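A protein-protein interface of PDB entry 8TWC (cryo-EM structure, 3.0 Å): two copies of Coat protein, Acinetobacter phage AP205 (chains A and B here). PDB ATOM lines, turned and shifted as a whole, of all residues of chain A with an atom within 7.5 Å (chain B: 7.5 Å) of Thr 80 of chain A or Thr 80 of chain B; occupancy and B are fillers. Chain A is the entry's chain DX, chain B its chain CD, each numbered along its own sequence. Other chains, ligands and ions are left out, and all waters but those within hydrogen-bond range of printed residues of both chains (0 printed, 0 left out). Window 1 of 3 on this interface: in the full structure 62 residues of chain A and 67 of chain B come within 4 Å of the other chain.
A ring nitrogen (ND1) of His 99 of chain A sits at hydrogen-bond distance from the side-chain hydroxyl of Ser 52 of chain B, 2.9 Å away. The backbone carbonyl oxygen (O) of Arg 79 of chain B is in hydrogen-bond range of the backbone NH (N) of Val 81 of chain A, 2.9 Å away. A ring nitrogen (NE2) of His 99 of chain A is in hydrogen-bond range of the side-chain hydroxyl (OG1) of Thr 80 of chain B. The backbone carbonyl oxygen (O) of Arg 79 of chain A sits at hydrogen-bond distance from the backbone NH (N) of Val 81 of chain B. A ring nitrogen (NE2) of His 99 of chain B lies within hydrogen-bond range of the side-chain hydroxyl of Thr 80 of chain A (3.2 Å).
The backbone carbonyl oxygen (O) of Tyr 50 of chain B lies within hydrogen-bond range of the backbone NH (N) of Thr 80 of chain B (2.6 Å). N of Ser 52 of chain B sits at hydrogen-bond distance from O of Ile 78 of chain B (2.7 Å). N of Tyr 50 of chain A is in hydrogen-bond range of O of Thr 80 of chain A (2.8 Å). The backbone carbonyl oxygen (O) of Ile 78 of chain A sits at hydrogen-bond distance from the backbone NH (N) of Ser 52 of chain A.
Phe 27 of chain A touches His 99 of chain B (CE1 to ND1, 3.7 Å). Tyr 50 of chain A touches His 99 of chain B. His 99 of chain B touches Ser 52 of chain A. O of Val 81 of chain B touches CA of Ile 78 of chain A, at 3.3 Å. Ile 78 of chain A touches His 99 of chain B. O of Arg 79 of chain A touches O of Arg 79 of chain B (3.8 Å). Val 81 of chain A touches Ile 78 of chain B (O to CA, 3.3 Å). Trp 96 of chain A touches Ile 78 of chain B. Val 103 of chain B touches Trp 96 of chain A (CG1 to CZ2, 3.6 Å). Lys 100 of chain A touches Lys 100 of chain B.
Of chain B, only Arg 79, Thr 80 and His 99 come within 4 Å of Thr 80 of chain A. Thr 80 of chain B touches just these residues of chain A: Arg 79, Thr 80 and His 99. Of the printed residues of chain B, Phe 27 of chain A touches His 99. Of the printed residues of chain A, Ser 52 of chain B touches His 99. Gly 48 of chain A touches none of the printed residues of chain B. The nearest residue of chain A that does not touch Thr 80 of chain B is Trp 96 of chain A (4.5 Å). The nearest printed residue of chain A that does not touch Lys 100 of chain B is Trp 96 of chain A (5.2 Å).
Of the 17 printed residues of chain B, 10 touch a printed residue of chain A. Hydrophobic or aromatic side chains of chain B within 4 Å of the printed part of chain A: Tyr 50, Ile 78, Val 81, Trp 96, His 99 and Val 103. Hydrophobic or aromatic side chains of chain A that line the printed part of chain B: Phe 27, Ile 78, Val 81, Trp 96, His 99 and Val 103. Among the printed residues, no Asp or Glu carboxylate lies within 4 Å of a Lys or Arg side-chain nitrogen of the other chain.
Tyr 50 of chain A touches His 99 of chain B, and with the chains exchanged His 99 of chain A touches Tyr 50 of chain B. Ile 78 of chain A touches Val 81 of chain B, and with the chains exchanged Val 81 of chain A touches Ile 78 of chain B. Arg 79 of chain B touches its own counterpart, Arg 79 of chain A. Trp 96 of chain A touches Val 103 of chain B, and with the chains exchanged Val 103 of chain A touches Trp 96 of chain B. Positions printed for both chains: 28, 30, 47, 48, 49, 50, 51, 52, 78, 79, 80, 81, 82, 96, 99, 100 and 103. Of the 23 pairs that touch across the chains among the printed residues, 21 have their exchanged pair printed and touching as well.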
ATOM      1  N   PHE A  27     -23.483 -21.796 -18.761  1.00  0.00           N
ATOM      2  CA  PHE A  27     -22.251 -21.821 -19.541  1.00  0.00           C
ATOM      3  C   PHE A  27     -21.083 -21.874 -18.570  1.00  0.00           C
ATOM      4  O   PHE A  27     -20.939 -20.987 -17.722  1.00  0.00           O
ATOM      5  CB  PHE A  27     -22.144 -20.601 -20.457  1.00  0.00           C
ATOM      6  CG  PHE A  27     -20.936 -20.620 -21.344  1.00  0.00           C
ATOM      7  CD1 PHE A  27     -20.914 -21.403 -22.484  1.00  0.00           C
ATOM      8  CD2 PHE A  27     -19.825 -19.859 -21.040  1.00  0.00           C
ATOM      9  CE1 PHE A  27     -19.807 -21.425 -23.304  1.00  0.00           C
ATOM     10  CE2 PHE A  27     -18.716 -19.878 -21.858  1.00  0.00           C
ATOM     11  CZ  PHE A  27     -18.705 -20.661 -22.989  1.00  0.00           C
ATOM     12  N   SER A  28     -20.250 -22.901 -18.697  1.00  0.00           N
ATOM     13  CA  SER A  28     -19.182 -23.168 -17.749  1.00  0.00           C
ATOM     14  C   SER A  28     -17.829 -23.075 -18.437  1.00  0.00           C
ATOM     15  O   SER A  28     -17.667 -23.496 -19.584  1.00  0.00           O
ATOM     16  CB  SER A  28     -19.340 -24.554 -17.117  1.00  0.00           C
ATOM     17  OG  SER A  28     -20.657 -24.747 -16.632  1.00  0.00           O
ATOM     18  N   SER A  30     -13.779 -23.937 -17.319  1.00  0.00           N
ATOM     19  CA  SER A  30     -12.850 -24.481 -16.336  1.00  0.00           C
ATOM     20  C   SER A  30     -11.473 -24.591 -16.970  1.00  0.00           C
ATOM     21  O   SER A  30     -11.331 -25.173 -18.049  1.00  0.00           O
ATOM     22  CB  SER A  30     -13.318 -25.846 -15.827  1.00  0.00           C
ATOM     23  OG  SER A  30     -12.259 -26.545 -15.197  1.00  0.00           O
ATOM     24  N   SER A  47      -5.382 -26.385 -20.273  1.00  0.00           N
ATOM     25  CA  SER A  47      -6.481 -27.120 -20.883  1.00  0.00           C
ATOM     26  C   SER A  47      -7.794 -26.438 -20.520  1.00  0.00           C
ATOM     27  O   SER A  47      -8.121 -26.304 -19.336  1.00  0.00           O
ATOM     28  CB  SER A  47      -6.482 -28.576 -20.425  1.00  0.00           C
ATOM     29  OG  SER A  47      -6.978 -28.692 -19.102  1.00  0.00           O
ATOM     30  N   GLY A  48      -8.543 -26.014 -21.533  1.00  0.00           N
ATOM     31  CA  GLY A  48      -9.773 -25.288 -21.294  1.00  0.00           C
ATOM     32  C   GLY A  48     -11.024 -26.050 -21.665  1.00  0.00           C
ATOM     33  O   GLY A  48     -11.216 -26.413 -22.828  1.00  0.00           O
ATOM     34  N   GLN A  49     -11.892 -26.287 -20.686  1.00  0.00           N
ATOM     35  CA  GLN A  49     -13.146 -26.997 -20.894  1.00  0.00           C
ATOM     36  C   GLN A  49     -14.290 -25.994 -20.836  1.00  0.00           C
ATOM     37  O   GLN A  49     -14.440 -25.274 -19.843  1.00  0.00           O
ATOM     38  CB  GLN A  49     -13.334 -28.092 -19.845  1.00  0.00           C
ATOM     39  CG  GLN A  49     -14.587 -28.925 -20.037  1.00  0.00           C
ATOM     40  CD  GLN A  49     -14.681 -30.066 -19.045  1.00  0.00           C
ATOM     41  OE1 GLN A  49     -13.806 -30.240 -18.197  1.00  0.00           O
ATOM     42  NE2 GLN A  49     -15.747 -30.852 -19.146  1.00  0.00           N
ATOM     43  N   TYR A  50     -15.091 -25.950 -21.897  1.00  0.00           N
ATOM     44  CA  TYR A  50     -16.223 -25.039 -21.998  1.00  0.00           C
ATOM     45  C   TYR A  50     -17.478 -25.851 -22.276  1.00  0.00           C
ATOM     46  O   TYR A  50     -17.527 -26.607 -23.252  1.00  0.00           O
ATOM     47  CB  TYR A  50     -15.992 -23.999 -23.094  1.00  0.00           C
ATOM     48  CG  TYR A  50     -14.651 -23.310 -22.998  1.00  0.00           C
ATOM     49  CD1 TYR A  50     -13.538 -23.817 -23.653  1.00  0.00           C
ATOM     50  CD2 TYR A  50     -14.497 -22.154 -22.247  1.00  0.00           C
ATOM     51  CE1 TYR A  50     -12.313 -23.191 -23.565  1.00  0.00           C
ATOM     52  CE2 TYR A  50     -13.275 -21.522 -22.153  1.00  0.00           C
ATOM     53  CZ  TYR A  50     -12.186 -22.045 -22.813  1.00  0.00           C
ATOM     54  OH  TYR A  50     -10.965 -21.418 -22.723  1.00  0.00           O
ATOM     55  N   VAL A  51     -18.488 -25.694 -21.423  1.00  0.00           N
ATOM     56  CA  VAL A  51     -19.719 -26.470 -21.500  1.00  0.00           C
ATOM     57  C   VAL A  51     -20.897 -25.509 -21.570  1.00  0.00           C
ATOM     58  O   VAL A  51     -21.003 -24.591 -20.751  1.00  0.00           O
ATOM     59  CB  VAL A  51     -19.876 -27.419 -20.297  1.00  0.00           C
ATOM     60  CG1 VAL A  51     -21.126 -28.268 -20.449  1.00  0.00           C
ATOM     61  CG2 VAL A  51     -18.644 -28.296 -20.146  1.00  0.00           C
ATOM     62  N   SER A  52     -21.774 -25.722 -22.544  1.00  0.00           N
ATOM     63  CA  SER A  52     -23.007 -24.961 -22.681  1.00  0.00           C
ATOM     64  C   SER A  52     -24.195 -25.907 -22.600  1.00  0.00           C
ATOM     65  O   SER A  52     -24.253 -26.909 -23.319  1.00  0.00           O
ATOM     66  CB  SER A  52     -23.036 -24.192 -24.003  1.00  0.00           C
ATOM     67  OG  SER A  52     -24.362 -23.858 -24.367  1.00  0.00           O
ATOM     68  N   ILE A  78     -23.209 -28.815 -25.425  1.00  0.00           N
ATOM     69  CA  ILE A  78     -22.089 -28.612 -26.337  1.00  0.00           C
ATOM     70  C   ILE A  78     -20.847 -28.378 -25.492  1.00  0.00           C
ATOM     71  O   ILE A  78     -20.799 -27.424 -24.707  1.00  0.00           O
ATOM     72  CB  ILE A  78     -22.328 -27.434 -27.292  1.00  0.00           C
ATOM     73  CG1 ILE A  78     -23.614 -27.654 -28.086  1.00  0.00           C
ATOM     74  CG2 ILE A  78     -21.148 -27.266 -28.230  1.00  0.00           C
ATOM     75  CD1 ILE A  78     -23.972 -26.511 -28.993  1.00  0.00           C
ATOM     76  N   ARG A  79     -19.848 -29.241 -25.648  1.00  0.00           N
ATOM     77  CA  ARG A  79     -18.653 -29.223 -24.817  1.00  0.00           C
ATOM     78  C   ARG A  79     -17.414 -29.179 -25.697  1.00  0.00           C
ATOM     79  O   ARG A  79     -17.257 -30.011 -26.595  1.00  0.00           O
ATOM     80  CB  ARG A  79     -18.616 -30.449 -23.901  1.00  0.00           C
ATOM     81  CG  ARG A  79     -17.449 -30.477 -22.936  1.00  0.00           C
ATOM     82  CD  ARG A  79     -17.448 -31.764 -22.129  1.00  0.00           C
ATOM     83  NE  ARG A  79     -17.045 -32.912 -22.933  1.00  0.00           N
ATOM     84  CZ  ARG A  79     -17.517 -34.141 -22.770  1.00  0.00           C
ATOM     85  NH1 ARG A  79     -18.413 -34.421 -21.838  1.00  0.00           N
ATOM     86  NH2 ARG A  79     -17.078 -35.115 -23.563  1.00  0.00           N
ATOM     87  N   THR A  80     -16.537 -28.213 -25.435  1.00  0.00           N
ATOM     88  CA  THR A  80     -15.285 -28.059 -26.162  1.00  0.00           C
ATOM     89  C   THR A  80     -14.118 -28.056 -25.186  1.00  0.00           C
ATOM     90  O   THR A  80     -14.180 -27.415 -24.132  1.00  0.00           O
ATOM     91  CB  THR A  80     -15.264 -26.767 -26.983  1.00  0.00           C
ATOM     92  OG1 THR A  80     -15.453 -25.644 -26.113  1.00  0.00           O
ATOM     93  CG2 THR A  80     -16.363 -26.782 -28.026  1.00  0.00           C
ATOM     94  N   VAL A  81     -13.056 -28.774 -25.540  1.00  0.00           N
ATOM     95  CA  VAL A  81     -11.836 -28.835 -24.744  1.00  0.00           C
ATOM     96  C   VAL A  81     -10.681 -28.381 -25.624  1.00  0.00           C
ATOM     97  O   VAL A  81     -10.463 -28.937 -26.707  1.00  0.00           O
ATOM     98  CB  VAL A  81     -11.581 -30.245 -24.191  1.00  0.00           C
ATOM     99  CG1 VAL A  81     -10.313 -30.262 -23.356  1.00  0.00           C
ATOM    100  CG2 VAL A  81     -12.769 -30.714 -23.370  1.00  0.00           C
ATOM    101  N   ILE A  82      -9.942 -27.378 -25.160  1.00  0.00           N
ATOM    102  CA  ILE A  82      -8.802 -26.829 -25.881  1.00  0.00           C
ATOM    103  C   ILE A  82      -7.566 -27.012 -25.015  1.00  0.00           C
ATOM    104  O   ILE A  82      -7.513 -26.514 -23.885  1.00  0.00           O
ATOM    105  CB  ILE A  82      -9.013 -25.350 -26.233  1.00  0.00           C
ATOM    106  CG1 ILE A  82     -10.260 -25.184 -27.100  1.00  0.00           C
ATOM    107  CG2 ILE A  82      -7.798 -24.798 -26.952  1.00  0.00           C
ATOM    108  CD1 ILE A  82     -10.672 -23.745 -27.300  1.00  0.00           C
ATOM    109  N   TRP A  96      -8.075 -23.161 -33.698  1.00  0.00           N
ATOM    110  CA  TRP A  96      -9.461 -23.018 -33.267  1.00  0.00           C
ATOM    111  C   TRP A  96     -10.343 -22.537 -34.411  1.00  0.00           C
ATOM    112  O   TRP A  96     -11.465 -23.021 -34.588  1.00  0.00           O
ATOM    113  CB  TRP A  96      -9.538 -22.062 -32.077  1.00  0.00           C
ATOM    114  CG  TRP A  96     -10.928 -21.801 -31.575  1.00  0.00           C
ATOM    115  CD1 TRP A  96     -11.488 -20.583 -31.329  1.00  0.00           C
ATOM    116  CD2 TRP A  96     -11.929 -22.774 -31.248  1.00  0.00           C
ATOM    117  NE1 TRP A  96     -12.771 -20.735 -30.873  1.00  0.00           N
ATOM    118  CE2 TRP A  96     -13.068 -22.069 -30.817  1.00  0.00           C
ATOM    119  CE3 TRP A  96     -11.974 -24.172 -31.280  1.00  0.00           C
ATOM    120  CZ2 TRP A  96     -14.237 -22.711 -30.422  1.00  0.00           C
ATOM    121  CZ3 TRP A  96     -13.137 -24.806 -30.888  1.00  0.00           C
ATOM    122  CH2 TRP A  96     -14.251 -24.077 -30.464  1.00  0.00           C
ATOM    123  N   HIS A  99     -10.791 -25.468 -36.791  1.00  0.00           N
ATOM    124  CA  HIS A  99     -11.739 -26.399 -36.194  1.00  0.00           C
ATOM    125  C   HIS A  99     -13.162 -25.874 -36.308  1.00  0.00           C
ATOM    126  O   HIS A  99     -14.094 -26.639 -36.580  1.00  0.00           O
ATOM    127  CB  HIS A  99     -11.365 -26.645 -34.732  1.00  0.00           C
ATOM    128  CG  HIS A  99     -12.343 -27.493 -33.984  1.00  0.00           C
ATOM    129  ND1 HIS A  99     -12.185 -28.854 -33.836  1.00  0.00           N
ATOM    130  CD2 HIS A  99     -13.481 -27.173 -33.325  1.00  0.00           C
ATOM    131  CE1 HIS A  99     -13.189 -29.336 -33.125  1.00  0.00           C
ATOM    132  NE2 HIS A  99     -13.989 -28.337 -32.803  1.00  0.00           N
ATOM    133  N   LYS A 100     -13.346 -24.570 -36.095  1.00  0.00           N
ATOM    134  CA  LYS A 100     -14.646 -23.948 -36.312  1.00  0.00           C
ATOM    135  C   LYS A 100     -15.158 -24.233 -37.710  1.00  0.00           C
ATOM    136  O   LYS A 100     -16.291 -24.690 -37.888  1.00  0.00           O
ATOM    137  CB  LYS A 100     -14.544 -22.440 -36.115  1.00  0.00           C
ATOM    138  CG  LYS A 100     -15.107 -21.897 -34.837  1.00  0.00           C
ATOM    139  CD  LYS A 100     -14.609 -20.482 -34.685  1.00  0.00           C
ATOM    140  CE  LYS A 100     -14.664 -20.017 -33.263  1.00  0.00           C
ATOM    141  NZ  LYS A 100     -13.854 -18.781 -33.123  1.00  0.00           N
ATOM    142  N   VAL A 103     -15.983 -28.032 -38.288  1.00  0.00           N
ATOM    143  CA  VAL A 103     -17.194 -28.456 -37.596  1.00  0.00           C
ATOM    144  C   VAL A 103     -18.418 -27.821 -38.241  1.00  0.00           C
ATOM    145  O   VAL A 103     -19.481 -28.440 -38.332  1.00  0.00           O
ATOM    146  CB  VAL A 103     -17.104 -28.131 -36.094  1.00  0.00           C
ATOM    147  CG1 VAL A 103     -18.408 -28.474 -35.396  1.00  0.00           C
ATOM    148  CG2 VAL A 103     -15.963 -28.904 -35.460  1.00  0.00           C
ATOM    149  N   SER B  28     -10.987 -35.814 -36.769  1.00  0.00           N
ATOM    150  CA  SER B  28     -11.853 -36.972 -36.616  1.00  0.00           C
ATOM    151  C   SER B  28     -13.255 -36.542 -36.211  1.00  0.00           C
ATOM    152  O   SER B  28     -13.433 -35.650 -35.375  1.00  0.00           O
ATOM    153  CB  SER B  28     -11.293 -37.947 -35.577  1.00  0.00           C
ATOM    154  OG  SER B  28     -12.155 -39.058 -35.406  1.00  0.00           O
ATOM    155  N   SER B  30     -16.862 -38.538 -35.087  1.00  0.00           N
ATOM    156  CA  SER B  30     -17.499 -39.800 -34.733  1.00  0.00           C
ATOM    157  C   SER B  30     -18.895 -39.516 -34.207  1.00  0.00           C
ATOM    158  O   SER B  30     -19.075 -38.623 -33.372  1.00  0.00           O
ATOM    159  CB  SER B  30     -16.677 -40.560 -33.690  1.00  0.00           C
ATOM    160  OG  SER B  30     -17.050 -40.187 -32.376  1.00  0.00           O
ATOM    161  N   SER B  47     -24.980 -37.682 -30.781  1.00  0.00           N
ATOM    162  CA  SER B  47     -23.857 -37.161 -30.006  1.00  0.00           C
ATOM    163  C   SER B  47     -22.613 -37.222 -30.884  1.00  0.00           C
ATOM    164  O   SER B  47     -21.943 -38.256 -30.958  1.00  0.00           O
ATOM    165  CB  SER B  47     -23.669 -37.952 -28.716  1.00  0.00           C
ATOM    166  OG  SER B  47     -23.273 -39.284 -28.989  1.00  0.00           O
ATOM    167  N   GLY B  48     -22.304 -36.109 -31.544  1.00  0.00           N
ATOM    168  CA  GLY B  48     -21.172 -36.037 -32.449  1.00  0.00           C
ATOM    169  C   GLY B  48     -19.939 -35.504 -31.742  1.00  0.00           C
ATOM    170  O   GLY B  48     -19.984 -34.457 -31.093  1.00  0.00           O
ATOM    171  N   GLN B  49     -18.840 -36.237 -31.883  1.00  0.00           N
ATOM    172  CA  GLN B  49     -17.557 -35.864 -31.302  1.00  0.00           C
ATOM    173  C   GLN B  49     -16.604 -35.491 -32.428  1.00  0.00           C
ATOM    174  O   GLN B  49     -16.325 -36.312 -33.307  1.00  0.00           O
ATOM    175  CB  GLN B  49     -16.986 -37.005 -30.463  1.00  0.00           C
ATOM    176  CG  GLN B  49     -15.701 -36.658 -29.736  1.00  0.00           C
ATOM    177  CD  GLN B  49     -15.002 -37.879 -29.178  1.00  0.00           C
ATOM    178  OE1 GLN B  49     -15.106 -38.178 -27.989  1.00  0.00           O
ATOM    179  NE2 GLN B  49     -14.283 -38.594 -30.036  1.00  0.00           N
ATOM    180  N   TYR B  50     -16.106 -34.257 -32.397  1.00  0.00           N
ATOM    181  CA  TYR B  50     -15.188 -33.748 -33.408  1.00  0.00           C
ATOM    182  C   TYR B  50     -13.876 -33.390 -32.726  1.00  0.00           C
ATOM    183  O   TYR B  50     -13.865 -32.602 -31.777  1.00  0.00           O
ATOM    184  CB  TYR B  50     -15.770 -32.530 -34.126  1.00  0.00           C
ATOM    185  CG  TYR B  50     -17.170 -32.722 -34.666  1.00  0.00           C
ATOM    186  CD1 TYR B  50     -17.388 -32.926 -36.019  1.00  0.00           C
ATOM    187  CD2 TYR B  50     -18.275 -32.670 -33.829  1.00  0.00           C
ATOM    188  CE1 TYR B  50     -18.663 -33.095 -36.519  1.00  0.00           C
ATOM    189  CE2 TYR B  50     -19.552 -32.837 -34.319  1.00  0.00           C
ATOM    190  CZ  TYR B  50     -19.740 -33.048 -35.665  1.00  0.00           C
ATOM    191  OH  TYR B  50     -21.012 -33.214 -36.159  1.00  0.00           O
ATOM    192  N   VAL B  51     -12.777 -33.961 -33.213  1.00  0.00           N
ATOM    193  CA  VAL B  51     -11.462 -33.783 -32.610  1.00  0.00           C
ATOM    194  C   VAL B  51     -10.494 -33.290 -33.675  1.00  0.00           C
ATOM    195  O   VAL B  51     -10.397 -33.885 -34.754  1.00  0.00           O
ATOM    196  CB  VAL B  51     -10.942 -35.088 -31.977  1.00  0.00           C
ATOM    197  CG1 VAL B  51      -9.600 -34.851 -31.306  1.00  0.00           C
ATOM    198  CG2 VAL B  51     -11.949 -35.636 -30.981  1.00  0.00           C
ATOM    199  N   SER B  52      -9.780 -32.212 -33.371  1.00  0.00           N
ATOM    200  CA  SER B  52      -8.719 -31.694 -34.221  1.00  0.00           C
ATOM    201  C   SER B  52      -7.394 -31.778 -33.478  1.00  0.00           C
ATOM    202  O   SER B  52      -7.278 -31.302 -32.345  1.00  0.00           O
ATOM    203  CB  SER B  52      -8.996 -30.246 -34.632  1.00  0.00           C
ATOM    204  OG  SER B  52     -10.166 -30.152 -35.422  1.00  0.00           O
ATOM    205  N   ILE B  78      -8.068 -30.069 -29.904  1.00  0.00           N
ATOM    206  CA  ILE B  78      -9.352 -29.392 -29.777  1.00  0.00           C
ATOM    207  C   ILE B  78     -10.438 -30.416 -30.066  1.00  0.00           C
ATOM    208  O   ILE B  78     -10.583 -30.861 -31.210  1.00  0.00           O
ATOM    209  CB  ILE B  78      -9.473 -28.193 -30.729  1.00  0.00           C
ATOM    210  CG1 ILE B  78      -8.357 -27.182 -30.465  1.00  0.00           C
ATOM    211  CG2 ILE B  78     -10.834 -27.538 -30.584  1.00  0.00           C
ATOM    212  CD1 ILE B  78      -8.386 -25.990 -31.388  1.00  0.00           C
ATOM    213  N   ARG B  79     -11.201 -30.785 -29.040  1.00  0.00           N
ATOM    214  CA  ARG B  79     -12.275 -31.758 -29.178  1.00  0.00           C
ATOM    215  C   ARG B  79     -13.600 -31.106 -28.814  1.00  0.00           C
ATOM    216  O   ARG B  79     -13.679 -30.346 -27.844  1.00  0.00           O
ATOM    217  CB  ARG B  79     -12.022 -33.002 -28.317  1.00  0.00           C
ATOM    218  CG  ARG B  79     -12.065 -32.778 -26.819  1.00  0.00           C
ATOM    219  CD  ARG B  79     -11.732 -34.060 -26.073  1.00  0.00           C
ATOM    220  NE  ARG B  79     -10.335 -34.441 -26.240  1.00  0.00           N
ATOM    221  CZ  ARG B  79      -9.815 -35.586 -25.817  1.00  0.00           C
ATOM    222  NH1 ARG B  79     -10.552 -36.492 -25.195  1.00  0.00           N
ATOM    223  NH2 ARG B  79      -8.524 -35.829 -26.026  1.00  0.00           N
ATOM    224  N   THR B  80     -14.628 -31.390 -29.607  1.00  0.00           N
ATOM    225  CA  THR B  80     -15.952 -30.811 -29.437  1.00  0.00           C
ATOM    226  C   THR B  80     -17.000 -31.913 -29.477  1.00  0.00           C
ATOM    227  O   THR B  80     -16.950 -32.797 -30.338  1.00  0.00           O
ATOM    228  CB  THR B  80     -16.243 -29.778 -30.532  1.00  0.00           C
ATOM    229  OG1 THR B  80     -15.293 -28.709 -30.446  1.00  0.00           O
ATOM    230  CG2 THR B  80     -17.647 -29.218 -30.389  1.00  0.00           C
ATOM    231  N   VAL B  81     -17.946 -31.858 -28.544  1.00  0.00           N
ATOM    232  CA  VAL B  81     -19.033 -32.825 -28.460  1.00  0.00           C
ATOM    233  C   VAL B  81     -20.347 -32.060 -28.497  1.00  0.00           C
ATOM    234  O   VAL B  81     -20.556 -31.140 -27.696  1.00  0.00           O
ATOM    235  CB  VAL B  81     -18.937 -33.686 -27.191  1.00  0.00           C
ATOM    236  CG1 VAL B  81     -20.152 -34.591 -27.074  1.00  0.00           C
ATOM    237  CG2 VAL B  81     -17.657 -34.504 -27.202  1.00  0.00           C
ATOM    238  N   ILE B  82     -21.227 -32.437 -29.418  1.00  0.00           N
ATOM    239  CA  ILE B  82     -22.547 -31.834 -29.551  1.00  0.00           C
ATOM    240  C   ILE B  82     -23.581 -32.935 -29.380  1.00  0.00           C
ATOM    241  O   ILE B  82     -23.583 -33.917 -30.133  1.00  0.00           O
ATOM    242  CB  ILE B  82     -22.714 -31.126 -30.903  1.00  0.00           C
ATOM    243  CG1 ILE B  82     -21.603 -30.098 -31.106  1.00  0.00           C
ATOM    244  CG2 ILE B  82     -24.075 -30.460 -30.988  1.00  0.00           C
ATOM    245  CD1 ILE B  82     -21.672 -29.382 -32.434  1.00  0.00           C
ATOM    246  N   TRP B  96     -25.088 -23.904 -31.071  1.00  0.00           N
ATOM    247  CA  TRP B  96     -23.704 -23.997 -31.526  1.00  0.00           C
ATOM    248  C   TRP B  96     -23.141 -22.619 -31.850  1.00  0.00           C
ATOM    249  O   TRP B  96     -21.997 -22.306 -31.506  1.00  0.00           O
ATOM    250  CB  TRP B  96     -23.611 -24.919 -32.740  1.00  0.00           C
ATOM    251  CG  TRP B  96     -22.279 -24.885 -33.423  1.00  0.00           C
ATOM    252  CD1 TRP B  96     -22.023 -24.473 -34.696  1.00  0.00           C
ATOM    253  CD2 TRP B  96     -21.020 -25.283 -32.871  1.00  0.00           C
ATOM    254  NE1 TRP B  96     -20.684 -24.587 -34.971  1.00  0.00           N
ATOM    255  CE2 TRP B  96     -20.046 -25.083 -33.865  1.00  0.00           C
ATOM    256  CE3 TRP B  96     -20.622 -25.789 -31.630  1.00  0.00           C
ATOM    257  CZ2 TRP B  96     -18.700 -25.370 -33.659  1.00  0.00           C
ATOM    258  CZ3 TRP B  96     -19.286 -26.073 -31.428  1.00  0.00           C
ATOM    259  CH2 TRP B  96     -18.341 -25.863 -32.437  1.00  0.00           C
ATOM    260  N   HIS B  99     -22.530 -20.831 -28.581  1.00  0.00           N
ATOM    261  CA  HIS B  99     -21.364 -21.411 -27.926  1.00  0.00           C
ATOM    262  C   HIS B  99     -20.078 -20.921 -28.573  1.00  0.00           C
ATOM    263  O   HIS B  99     -19.102 -20.605 -27.884  1.00  0.00           O
ATOM    264  CB  HIS B  99     -21.449 -22.936 -27.976  1.00  0.00           C
ATOM    265  CG  HIS B  99     -20.311 -23.629 -27.300  1.00  0.00           C
ATOM    266  ND1 HIS B  99     -20.310 -23.916 -25.952  1.00  0.00           N
ATOM    267  CD2 HIS B  99     -19.138 -24.099 -27.786  1.00  0.00           C
ATOM    268  CE1 HIS B  99     -19.184 -24.530 -25.636  1.00  0.00           C
ATOM    269  NE2 HIS B  99     -18.455 -24.652 -26.731  1.00  0.00           N
ATOM    270  N   LYS B 100     -20.059 -20.853 -29.906  1.00  0.00           N
ATOM    271  CA  LYS B 100     -18.894 -20.320 -30.603  1.00  0.00           C
ATOM    272  C   LYS B 100     -18.642 -18.875 -30.204  1.00  0.00           C
ATOM    273  O   LYS B 100     -17.498 -18.476 -29.960  1.00  0.00           O
ATOM    274  CB  LYS B 100     -19.086 -20.429 -32.115  1.00  0.00           C
ATOM    275  CG  LYS B 100     -18.890 -21.821 -32.679  1.00  0.00           C
ATOM    276  CD  LYS B 100     -18.734 -21.770 -34.189  1.00  0.00           C
ATOM    277  CE  LYS B 100     -20.022 -21.340 -34.863  1.00  0.00           C
ATOM    278  NZ  LYS B 100     -19.837 -21.130 -36.325  1.00  0.00           N
ATOM    279  N   VAL B 103     -17.223 -18.817 -26.560  1.00  0.00           N
ATOM    280  CA  VAL B 103     -15.844 -19.292 -26.521  1.00  0.00           C
ATOM    281  C   VAL B 103     -14.918 -18.272 -27.165  1.00  0.00           C
ATOM    282  O   VAL B 103     -13.783 -18.081 -26.719  1.00  0.00           O
ATOM    283  CB  VAL B 103     -15.726 -20.676 -27.184  1.00  0.00           C
ATOM    284  CG1 VAL B 103     -14.276 -21.117 -27.238  1.00  0.00           C
ATOM    285  CG2 VAL B 103     -16.542 -21.696 -26.414  1.00  0.00           C
